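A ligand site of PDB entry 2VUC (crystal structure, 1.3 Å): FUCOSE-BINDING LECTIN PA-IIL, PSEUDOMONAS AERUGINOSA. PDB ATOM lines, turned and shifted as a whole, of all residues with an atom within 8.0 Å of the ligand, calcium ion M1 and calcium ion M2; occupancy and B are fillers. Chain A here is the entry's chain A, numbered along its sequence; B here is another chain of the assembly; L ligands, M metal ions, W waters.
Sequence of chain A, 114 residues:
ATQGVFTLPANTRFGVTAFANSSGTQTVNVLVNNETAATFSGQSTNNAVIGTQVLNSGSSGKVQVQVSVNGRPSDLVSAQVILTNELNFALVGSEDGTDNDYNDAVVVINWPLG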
ATOM      1  N   ALA A  20     -21.147 -17.100 -12.083  1.00  0.00           N
ATOM      2  CA  ALA A  20     -21.542 -15.820 -12.706  1.00  0.00           C
ATOM      3  C   ALA A  20     -22.425 -14.998 -11.778  1.00  0.00           C
ATOM      4  O   ALA A  20     -23.299 -15.526 -11.084  1.00  0.00           O
ATOM      5  CB  ALA A  20     -22.264 -16.078 -14.031  1.00  0.00           C
ATOM      6  N   ASN A  21     -22.157 -13.682 -11.798  1.00  0.00           N
ATOM      7  CA  ASN A  21     -22.906 -12.705 -11.014  1.00  0.00           C
ATOM      8  C   ASN A  21     -22.993 -11.387 -11.784  1.00  0.00           C
ATOM      9  O   ASN A  21     -22.318 -10.408 -11.432  1.00  0.00           O
ATOM     10  CB  ASN A  21     -22.237 -12.440  -9.664  1.00  0.00           C
ATOM     11  CG  ASN A  21     -22.312 -13.626  -8.734  1.00  0.00           C
ATOM     12  OD1 ASN A  21     -23.350 -13.884  -8.114  1.00  0.00           O
ATOM     13  ND2 ASN A  21     -21.178 -14.352  -8.615  1.00  0.00           N
ATOM     14  N   SER A  22     -23.791 -11.390 -12.849  1.00  0.00           N
ATOM     15  CA  SER A  22     -23.847 -10.212 -13.706  1.00  0.00           C
ATOM     16  C   SER A  22     -25.045 -10.331 -14.636  1.00  0.00           C
ATOM     17  O   SER A  22     -25.507 -11.432 -14.968  1.00  0.00           O
ATOM     18  CB  SER A  22     -22.571 -10.138 -14.565  1.00  0.00           C
ATOM     19  OG  SER A  22     -22.691  -9.075 -15.519  1.00  0.00           O
ATOM     20  N   SER A  23     -25.527  -9.181 -15.117  1.00  0.00           N
ATOM     21  CA  SER A  23     -26.545  -9.172 -16.188  1.00  0.00           C
ATOM     22  C   SER A  23     -25.993  -9.790 -17.467  1.00  0.00           C
ATOM     23  O   SER A  23     -26.772 -10.346 -18.272  1.00  0.00           O
ATOM     24  CB  SER A  23     -27.001  -7.733 -16.511  1.00  0.00           C
ATOM     25  OG  SER A  23     -25.932  -6.972 -17.014  1.00  0.00           O
ATOM     26  N   GLY A  24     -24.675  -9.690 -17.685  1.00  0.00           N
ATOM     27  CA  GLY A  24     -24.085 -10.133 -18.954  1.00  0.00           C
ATOM     28  C   GLY A  24     -23.602 -11.565 -18.972  1.00  0.00           C
ATOM     29  O   GLY A  24     -23.150 -12.120 -17.952  1.00  0.00           O
ATOM     30  N   GLN A  26     -21.143 -14.361 -19.342  1.00  0.00           N
ATOM     31  CA  GLN A  26     -19.676 -14.488 -19.144  1.00  0.00           C
ATOM     32  C   GLN A  26     -19.127 -15.617 -19.997  1.00  0.00           C
ATOM     33  O   GLN A  26     -19.700 -16.717 -19.997  1.00  0.00           O
ATOM     34  CB  GLN A  26     -19.395 -14.837 -17.649  1.00  0.00           C
ATOM     35  CG  GLN A  26     -20.123 -13.953 -16.651  1.00  0.00           C
ATOM     36  CD  GLN A  26     -19.571 -12.545 -16.630  1.00  0.00           C
ATOM     37  OE1 GLN A  26     -18.370 -12.347 -16.442  1.00  0.00           O
ATOM     38  NE2 GLN A  26     -20.436 -11.568 -16.809  1.00  0.00           N
ATOM     39  N   GLN A  43     -24.958 -17.161 -17.927  1.00  0.00           N
ATOM     40  CA  GLN A  43     -25.440 -15.916 -17.355  1.00  0.00           C
ATOM     41  C   GLN A  43     -26.195 -16.220 -16.082  1.00  0.00           C
ATOM     42  O   GLN A  43     -27.063 -17.111 -16.061  1.00  0.00           O
ATOM     43  CB  GLN A  43     -26.316 -15.153 -18.360  1.00  0.00           C
ATOM     44  CG  GLN A  43     -26.746 -13.757 -17.912  1.00  0.00           C
ATOM     45  CD  GLN A  43     -27.901 -13.761 -16.925  1.00  0.00           C
ATOM     46  OE1 GLN A  43     -28.862 -14.527 -17.101  1.00  0.00           O
ATOM     47  NE2 GLN A  43     -27.858 -12.926 -15.892  1.00  0.00           N
ATOM     48  N   SER A  44     -25.864 -15.486 -15.026  1.00  0.00           N
ATOM     49  CA  SER A  44     -26.573 -15.622 -13.754  1.00  0.00           C
ATOM     50  C   SER A  44     -26.312 -14.379 -12.930  1.00  0.00           C
ATOM     51  O   SER A  44     -25.200 -13.830 -13.009  1.00  0.00           O
ATOM     52  CB  SER A  44     -26.053 -16.854 -12.995  1.00  0.00           C
ATOM     53  OG  SER A  44     -26.680 -16.962 -11.719  1.00  0.00           O
ATOM     54  N   THR A  45     -27.276 -13.944 -12.140  1.00  0.00           N
ATOM     55  CA  THR A  45     -27.048 -12.957 -11.081  1.00  0.00           C
ATOM     56  C   THR A  45     -27.141 -13.600  -9.708  1.00  0.00           C
ATOM     57  O   THR A  45     -27.232 -12.916  -8.695  1.00  0.00           O
ATOM     58  CB  THR A  45     -28.032 -11.770 -11.154  1.00  0.00           C
ATOM     59  OG1 THR A  45     -29.353 -12.291 -11.282  1.00  0.00           O
ATOM     60  CG2 THR A  45     -27.737 -10.900 -12.345  1.00  0.00           C
ATOM     61  N   VAL A  69     -16.910 -10.480 -21.707  1.00  0.00           N
ATOM     62  CA  VAL A  69     -18.337 -10.188 -21.549  1.00  0.00           C
ATOM     63  C   VAL A  69     -18.684  -9.079 -22.537  1.00  0.00           C
ATOM     64  O   VAL A  69     -17.975  -8.071 -22.624  1.00  0.00           O
ATOM     65  CB  VAL A  69     -18.672  -9.667 -20.133  1.00  0.00           C
ATOM     66  CG1 VAL A  69     -20.188  -9.464 -19.959  1.00  0.00           C
ATOM     67  CG2 VAL A  69     -18.141 -10.600 -19.086  1.00  0.00           C
ATOM     68  N   SER A  94     -13.450 -10.879 -11.532  1.00  0.00           N
ATOM     69  CA  SER A  94     -13.447 -10.146 -12.792  1.00  0.00           C
ATOM     70  C   SER A  94     -14.566  -9.125 -12.784  1.00  0.00           C
ATOM     71  O   SER A  94     -15.633  -9.342 -12.183  1.00  0.00           O
ATOM     72  CB  SER A  94     -13.558 -11.070 -13.999  1.00  0.00           C
ATOM     73  OG  SER A  94     -14.807 -11.743 -14.017  1.00  0.00           O
ATOM     74  N   GLU A  95     -14.303  -7.999 -13.474  1.00  0.00           N
ATOM     75  CA  GLU A  95     -15.253  -6.888 -13.543  1.00  0.00           C
ATOM     76  C   GLU A  95     -15.568  -6.555 -15.005  1.00  0.00           C
ATOM     77  O   GLU A  95     -14.648  -6.246 -15.796  1.00  0.00           O
ATOM     78  CB  GLU A  95     -14.674  -5.663 -12.822  1.00  0.00           C
ATOM     79  CG  GLU A  95     -15.575  -4.432 -12.898  1.00  0.00           C
ATOM     80  CD  GLU A  95     -16.962  -4.718 -12.369  1.00  0.00           C
ATOM     81  OE1 GLU A  95     -17.103  -5.288 -11.257  1.00  0.00           O
ATOM     82  OE2 GLU A  95     -17.957  -4.390 -13.056  1.00  0.00           O
ATOM     83  N   ASP A  96     -16.855  -6.639 -15.331  1.00  0.00           N
ATOM     84  CA  ASP A  96     -17.313  -6.401 -16.702  1.00  0.00           C
ATOM     85  C   ASP A  96     -17.918  -5.025 -16.912  1.00  0.00           C
ATOM     86  O   ASP A  96     -18.324  -4.700 -18.040  1.00  0.00           O
ATOM     87  CB  ASP A  96     -18.291  -7.511 -17.155  1.00  0.00           C
ATOM     88  CG  ASP A  96     -19.597  -7.516 -16.402  1.00  0.00           C
ATOM     89  OD1 ASP A  96     -20.041  -6.471 -15.904  1.00  0.00           O
ATOM     90  OD2 ASP A  96     -20.225  -8.611 -16.357  1.00  0.00           O
ATOM     91  N   GLY A  97     -17.999  -4.243 -15.842  1.00  0.00           N
ATOM     92  CA  GLY A  97     -18.780  -3.005 -15.891  1.00  0.00           C
ATOM     93  C   GLY A  97     -18.119  -1.909 -15.075  1.00  0.00           C
ATOM     94  O   GLY A  97     -16.894  -1.709 -15.148  1.00  0.00           O
ATOM     95  N   THR A  98     -18.938  -1.238 -14.273  1.00  0.00           N
ATOM     96  CA  THR A  98     -18.514   0.003 -13.621  1.00  0.00           C
ATOM     97  C   THR A  98     -18.622  -0.071 -12.107  1.00  0.00           C
ATOM     98  O   THR A  98     -18.078   0.800 -11.400  1.00  0.00           O
ATOM     99  CB  THR A  98     -19.357   1.191 -14.102  1.00  0.00           C
ATOM    100  OG1 THR A  98     -20.730   0.913 -13.816  1.00  0.00           O
ATOM    101  CG2 THR A  98     -19.180   1.400 -15.598  1.00  0.00           C
ATOM    102  N   ASP A  99     -19.334  -1.059 -11.549  1.00  0.00           N
ATOM    103  CA  ASP A  99     -19.593  -1.074 -10.098  1.00  0.00           C
ATOM    104  C   ASP A  99     -18.441  -1.628  -9.249  1.00  0.00           C
ATOM    105  O   ASP A  99     -18.456  -1.485  -8.028  1.00  0.00           O
ATOM    106  CB  ASP A  99     -20.912  -1.779  -9.732  1.00  0.00           C
ATOM    107  CG  ASP A  99     -20.887  -3.284  -9.996  1.00  0.00           C
ATOM    108  OD1 ASP A  99     -19.946  -3.781 -10.645  1.00  0.00           O
ATOM    109  OD2 ASP A  99     -21.845  -3.951  -9.567  1.00  0.00           O
ATOM    110  N   ASN A 100     -17.466  -2.227  -9.909  1.00  0.00           N
ATOM    111  CA  ASN A 100     -16.279  -2.771  -9.228  1.00  0.00           C
ATOM    112  C   ASN A 100     -16.578  -3.758  -8.115  1.00  0.00           C
ATOM    113  O   ASN A 100     -15.900  -3.775  -7.079  1.00  0.00           O
ATOM    114  CB  ASN A 100     -15.361  -1.620  -8.777  1.00  0.00           C
ATOM    115  CG  ASN A 100     -14.820  -0.858  -9.961  1.00  0.00           C
ATOM    116  OD1 ASN A 100     -14.694  -1.394 -11.071  1.00  0.00           O
ATOM    117  ND2 ASN A 100     -14.499   0.415  -9.736  1.00  0.00           N
ATOM    118  N   ASP A 101     -17.595  -4.610  -8.311  1.00  0.00           N
ATOM    119  CA  ASP A 101     -17.797  -5.705  -7.384  1.00  0.00           C
ATOM    120  C   ASP A 101     -16.876  -6.894  -7.687  1.00  0.00           C
ATOM    121  O   ASP A 101     -16.644  -7.719  -6.796  1.00  0.00           O
ATOM    122  CB  ASP A 101     -19.283  -6.113  -7.223  1.00  0.00           C
ATOM    123  CG  ASP A 101     -19.941  -6.670  -8.501  1.00  0.00           C
ATOM    124  OD1 ASP A 101     -19.307  -6.680  -9.579  1.00  0.00           O
ATOM    125  OD2 ASP A 101     -21.116  -7.103  -8.393  1.00  0.00           O
ATOM    126  N   TYR A 102     -16.309  -6.942  -8.892  1.00  0.00           N
ATOM    127  CA  TYR A 102     -15.346  -7.964  -9.277  1.00  0.00           C
ATOM    128  C   TYR A 102     -15.826  -9.434  -9.114  1.00  0.00           C
ATOM    129  O   TYR A 102     -15.009 -10.358  -9.026  1.00  0.00           O
ATOM    130  CB  TYR A 102     -13.963  -7.734  -8.602  1.00  0.00           C
ATOM    131  CG  TYR A 102     -13.185  -6.673  -9.345  1.00  0.00           C
ATOM    132  CD1 TYR A 102     -12.352  -7.013 -10.394  1.00  0.00           C
ATOM    133  CD2 TYR A 102     -13.405  -5.317  -9.078  1.00  0.00           C
ATOM    134  CE1 TYR A 102     -11.693  -6.039 -11.114  1.00  0.00           C
ATOM    135  CE2 TYR A 102     -12.767  -4.333  -9.850  1.00  0.00           C
ATOM    136  CZ  TYR A 102     -11.918  -4.726 -10.843  1.00  0.00           C
ATOM    137  OH  TYR A 102     -11.316  -3.720 -11.597  1.00  0.00           O
ATOM    138  N   ASN A 103     -17.156  -9.641  -9.127  1.00  0.00           N
ATOM    139  CA  ASN A 103     -17.707 -10.989  -8.976  1.00  0.00           C
ATOM    140  C   ASN A 103     -18.408 -11.452 -10.236  1.00  0.00           C
ATOM    141  O   ASN A 103     -19.101 -12.457 -10.228  1.00  0.00           O
ATOM    142  CB  ASN A 103     -18.681 -11.031  -7.797  1.00  0.00           C
ATOM    143  CG  ASN A 103     -19.973 -10.299  -8.098  1.00  0.00           C
ATOM    144  OD1 ASN A 103     -20.107  -9.737  -9.197  1.00  0.00           O
ATOM    145  ND2 ASN A 103     -20.923 -10.338  -7.181  1.00  0.00           N
ATOM    146  N   ASP A 104     -18.224 -10.729 -11.341  1.00  0.00           N
ATOM    147  CA  ASP A 104     -19.110 -10.933 -12.507  1.00  0.00           C
ATOM    148  C   ASP A 104     -18.885 -12.313 -13.082  1.00  0.00           C
ATOM    149  O   ASP A 104     -19.840 -13.017 -13.433  1.00  0.00           O
ATOM    150  CB  ASP A 104     -18.873  -9.806 -13.516  1.00  0.00           C
ATOM    151  CG  ASP A 104     -19.217  -8.445 -12.928  1.00  0.00           C
ATOM    152  OD1 ASP A 104     -20.160  -8.333 -12.111  1.00  0.00           O
ATOM    153  OD2 ASP A 104     -18.510  -7.470 -13.265  1.00  0.00           O
ATOM    154  N   ALA A 105     -17.611 -12.721 -13.195  1.00  0.00           N
ATOM    155  CA  ALA A 105     -17.255 -14.153 -13.231  1.00  0.00           C
ATOM    156  C   ALA A 105     -16.246 -14.353 -12.127  1.00  0.00           C
ATOM    157  O   ALA A 105     -15.268 -13.569 -12.027  1.00  0.00           O
ATOM    158  CB  ALA A 105     -16.645 -14.552 -14.563  1.00  0.00           C
ATOM    159  N   GLU B  86     -12.664  -5.865  -1.772  1.00  0.00           N
ATOM    160  CA  GLU B  86     -14.082  -6.021  -2.024  1.00  0.00           C
ATOM    161  C   GLU B  86     -14.528  -7.465  -2.189  1.00  0.00           C
ATOM    162  O   GLU B  86     -15.608  -7.818  -1.721  1.00  0.00           O
ATOM    163  CB  GLU B  86     -14.443  -5.200  -3.279  1.00  0.00           C
ATOM    164  CG  GLU B  86     -15.670  -5.660  -4.079  1.00  0.00           C
ATOM    165  CD  GLU B  86     -16.924  -5.122  -3.476  1.00  0.00           C
ATOM    166  OE1 GLU B  86     -16.823  -4.314  -2.531  1.00  0.00           O
ATOM    167  OE2 GLU B  86     -18.016  -5.493  -3.949  1.00  0.00           O
ATOM    168  N   PRO B 112     -19.355 -10.612  -2.334  1.00  0.00           N
ATOM    169  CA  PRO B 112     -20.799 -10.517  -2.564  1.00  0.00           C
ATOM    170  C   PRO B 112     -21.201 -11.252  -3.813  1.00  0.00           C
ATOM    171  O   PRO B 112     -20.374 -11.564  -4.665  1.00  0.00           O
ATOM    172  CB  PRO B 112     -21.031  -8.988  -2.712  1.00  0.00           C
ATOM    173  CG  PRO B 112     -19.769  -8.517  -3.342  1.00  0.00           C
ATOM    174  CD  PRO B 112     -18.653  -9.354  -2.682  1.00  0.00           C
ATOM    175  N   LEU B 113     -22.506 -11.462  -3.915  1.00  0.00           N
ATOM    176  CA  LEU B 113     -23.130 -12.005  -5.115  1.00  0.00           C
ATOM    177  C   LEU B 113     -23.849 -10.913  -5.879  1.00  0.00           C
ATOM    178  O   LEU B 113     -23.897  -9.771  -5.437  1.00  0.00           O
ATOM    179  CB  LEU B 113     -24.132 -13.110  -4.754  1.00  0.00           C
ATOM    180  CG  LEU B 113     -23.588 -14.260  -3.889  1.00  0.00           C
ATOM    181  CD1 LEU B 113     -24.668 -15.331  -3.748  1.00  0.00           C
ATOM    182  CD2 LEU B 113     -22.259 -14.841  -4.438  1.00  0.00           C
ATOM    183  N   GLY B 114     -24.392 -11.261  -7.041  1.00  0.00           N
ATOM    184  CA  GLY B 114     -25.279 -10.361  -7.774  1.00  0.00           C
ATOM    185  C   GLY B 114     -24.570  -9.517  -8.791  1.00  0.00           C
ATOM    186  O   GLY B 114     -23.335  -9.299  -8.749  1.00  0.00           O
ATOM    187  OXT GLY B 114     -25.285  -8.990  -9.667  1.00  0.00           O
HETATM  188  C1  LIG L   1     -23.424  -6.028 -14.385  1.00  0.00           C
HETATM  189  C2  LIG L   1     -22.355  -6.241 -13.325  1.00  0.00           C
HETATM  190  C3  LIG L   1     -22.829  -5.756 -11.974  1.00  0.00           C
HETATM  191  C4  LIG L   1     -24.123  -6.401 -11.586  1.00  0.00           C
HETATM  192  C5  LIG L   1     -25.168  -6.219 -12.698  1.00  0.00           C
HETATM  193  C6  LIG L   1     -26.450  -6.994 -12.409  1.00  0.00           C
HETATM  194  O1  LIG L   1     -23.652  -4.601 -14.475  1.00  0.00           O
HETATM  195  O2  LIG L   1     -21.109  -5.598 -13.669  1.00  0.00           O
HETATM  196  O3  LIG L   1     -21.790  -6.120 -11.032  1.00  0.00           O
HETATM  197  O4  LIG L   1     -23.829  -7.790 -11.359  1.00  0.00           O
HETATM  198  O5  LIG L   1     -24.627  -6.651 -13.962  1.00  0.00           O
HETATM  199 CA    CA M   1     -21.699  -8.422 -10.311  1.00  0.00          CA
HETATM  200 CA    CA M   2     -19.465  -5.803 -11.767  1.00  0.00          CA
HETATM  201  O   HOH W   1     -25.084  -4.427 -16.801  1.00  0.00           O
HETATM  202  O   HOH W   2     -21.344  -2.573 -13.500  1.00  0.00           O
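Within 4 Å of the ligand: Asn 21, Ser 22, Ser 23, Glu 95, Asp 96, Asp 99, Asp 101, Asp 104 and Gly 114 of chain B.
Calcium ion M1 is bound by OD1 of Asn 103 (2.3 Å), O of Asn 21 (2.4 Å), OD1 of Asp 104 (2.4 Å), OD2 of Asp 101 (2.4 Å), O3 of the ligand (2.4 Å), O of Gly 114 of chain B (2.4 Å) and O4 of the ligand (2.5 Å).
Calcium ion M1 has seven donor atoms within binding distance.
Slightly farther from calcium ion M1 lies OD1 of Asp 101 (3.0 Å).
The side-chain carboxylate of Asp 96 sits close to an oxygen (O2) of the ligand, at 2.6 Å.
N of Ser 23 is in hydrogen-bond range of O5 of the ligand (2.9 Å).
The side-chain hydroxyl (OG) of Ser 23 is in hydrogen-bond range of an oxygen (O5) of the ligand, 3.3 Å away.
The side-chain hydroxyl (OG) of Ser 22 sits close to an oxygen (O5) of the ligand.
Calcium ion M2 is bound by the side-chain carboxylate (OD1) of Asp 99 (2.4 Å), the side-chain carboxylate (OD1) of Asp 101 (2.4 Å), the side-chain carboxylate (OE2) of Glu 95 (2.4 Å), the side-chain carboxylate (OD2) of Asp 104 (2.4 Å), an oxygen (O3) of the ligand (2.5 Å), the side-chain carboxylate (OE1) of Glu 95 (2.5 Å), an oxygen (O2) of the ligand (2.5 Å) and the side-chain carboxylate (OD1) of Asp 104 (2.6 Å).
Calcium ion M2 has eight donor atoms within binding distance.
Five residues have an atom within 4 Å of calcium ion M1: Asn 21, Asp 101, Asn 103, Asp 104 and Gly 114 of chain B.
Water W1 lies within hydrogen-bond range of the side-chain hydroxyl of Ser 23 (2.7 Å) and an oxygen (O1) of the ligand (2.7 Å).
Water W2 lies within hydrogen-bond range of the backbone NH of Thr 98, the backbone NH of Asp 99 and an oxygen (O1) of the ligand.
Of the 26 residues printed, 4 come within 4 Å of calcium ion M2.
The backbone NH of Asn 103 lies within hydrogen-bond range of the backbone carbonyl oxygen of Ser 94, at 3.4 Å.
The backbone NH of Asn 21 sits close to the backbone carbonyl oxygen of Ser 44 (3.3 Å).
O of Asp 104 lies close to OE1 of Gln 26 (3.4 Å).
The side-chain carboxylate of Glu 95 sits close to the backbone NH of Gly 97 (2.8 Å).
The side-chain carboxylate (OE1) of Glu 95 sits close to the backbone NH (N) of Tyr 102, at 3.0 Å.
OE1 of Glu 95 sits close to N of Asn 100 (3.4 Å).
The side-chain amide nitrogen (NE2) of Gln 26 lies within hydrogen-bond range of the side-chain carboxylate (OD2) of Asp 96 (3.0 Å).
The backbone NH (N) of Gly 24 is in hydrogen-bond range of the side-chain hydroxyl (OG) of Ser 22.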
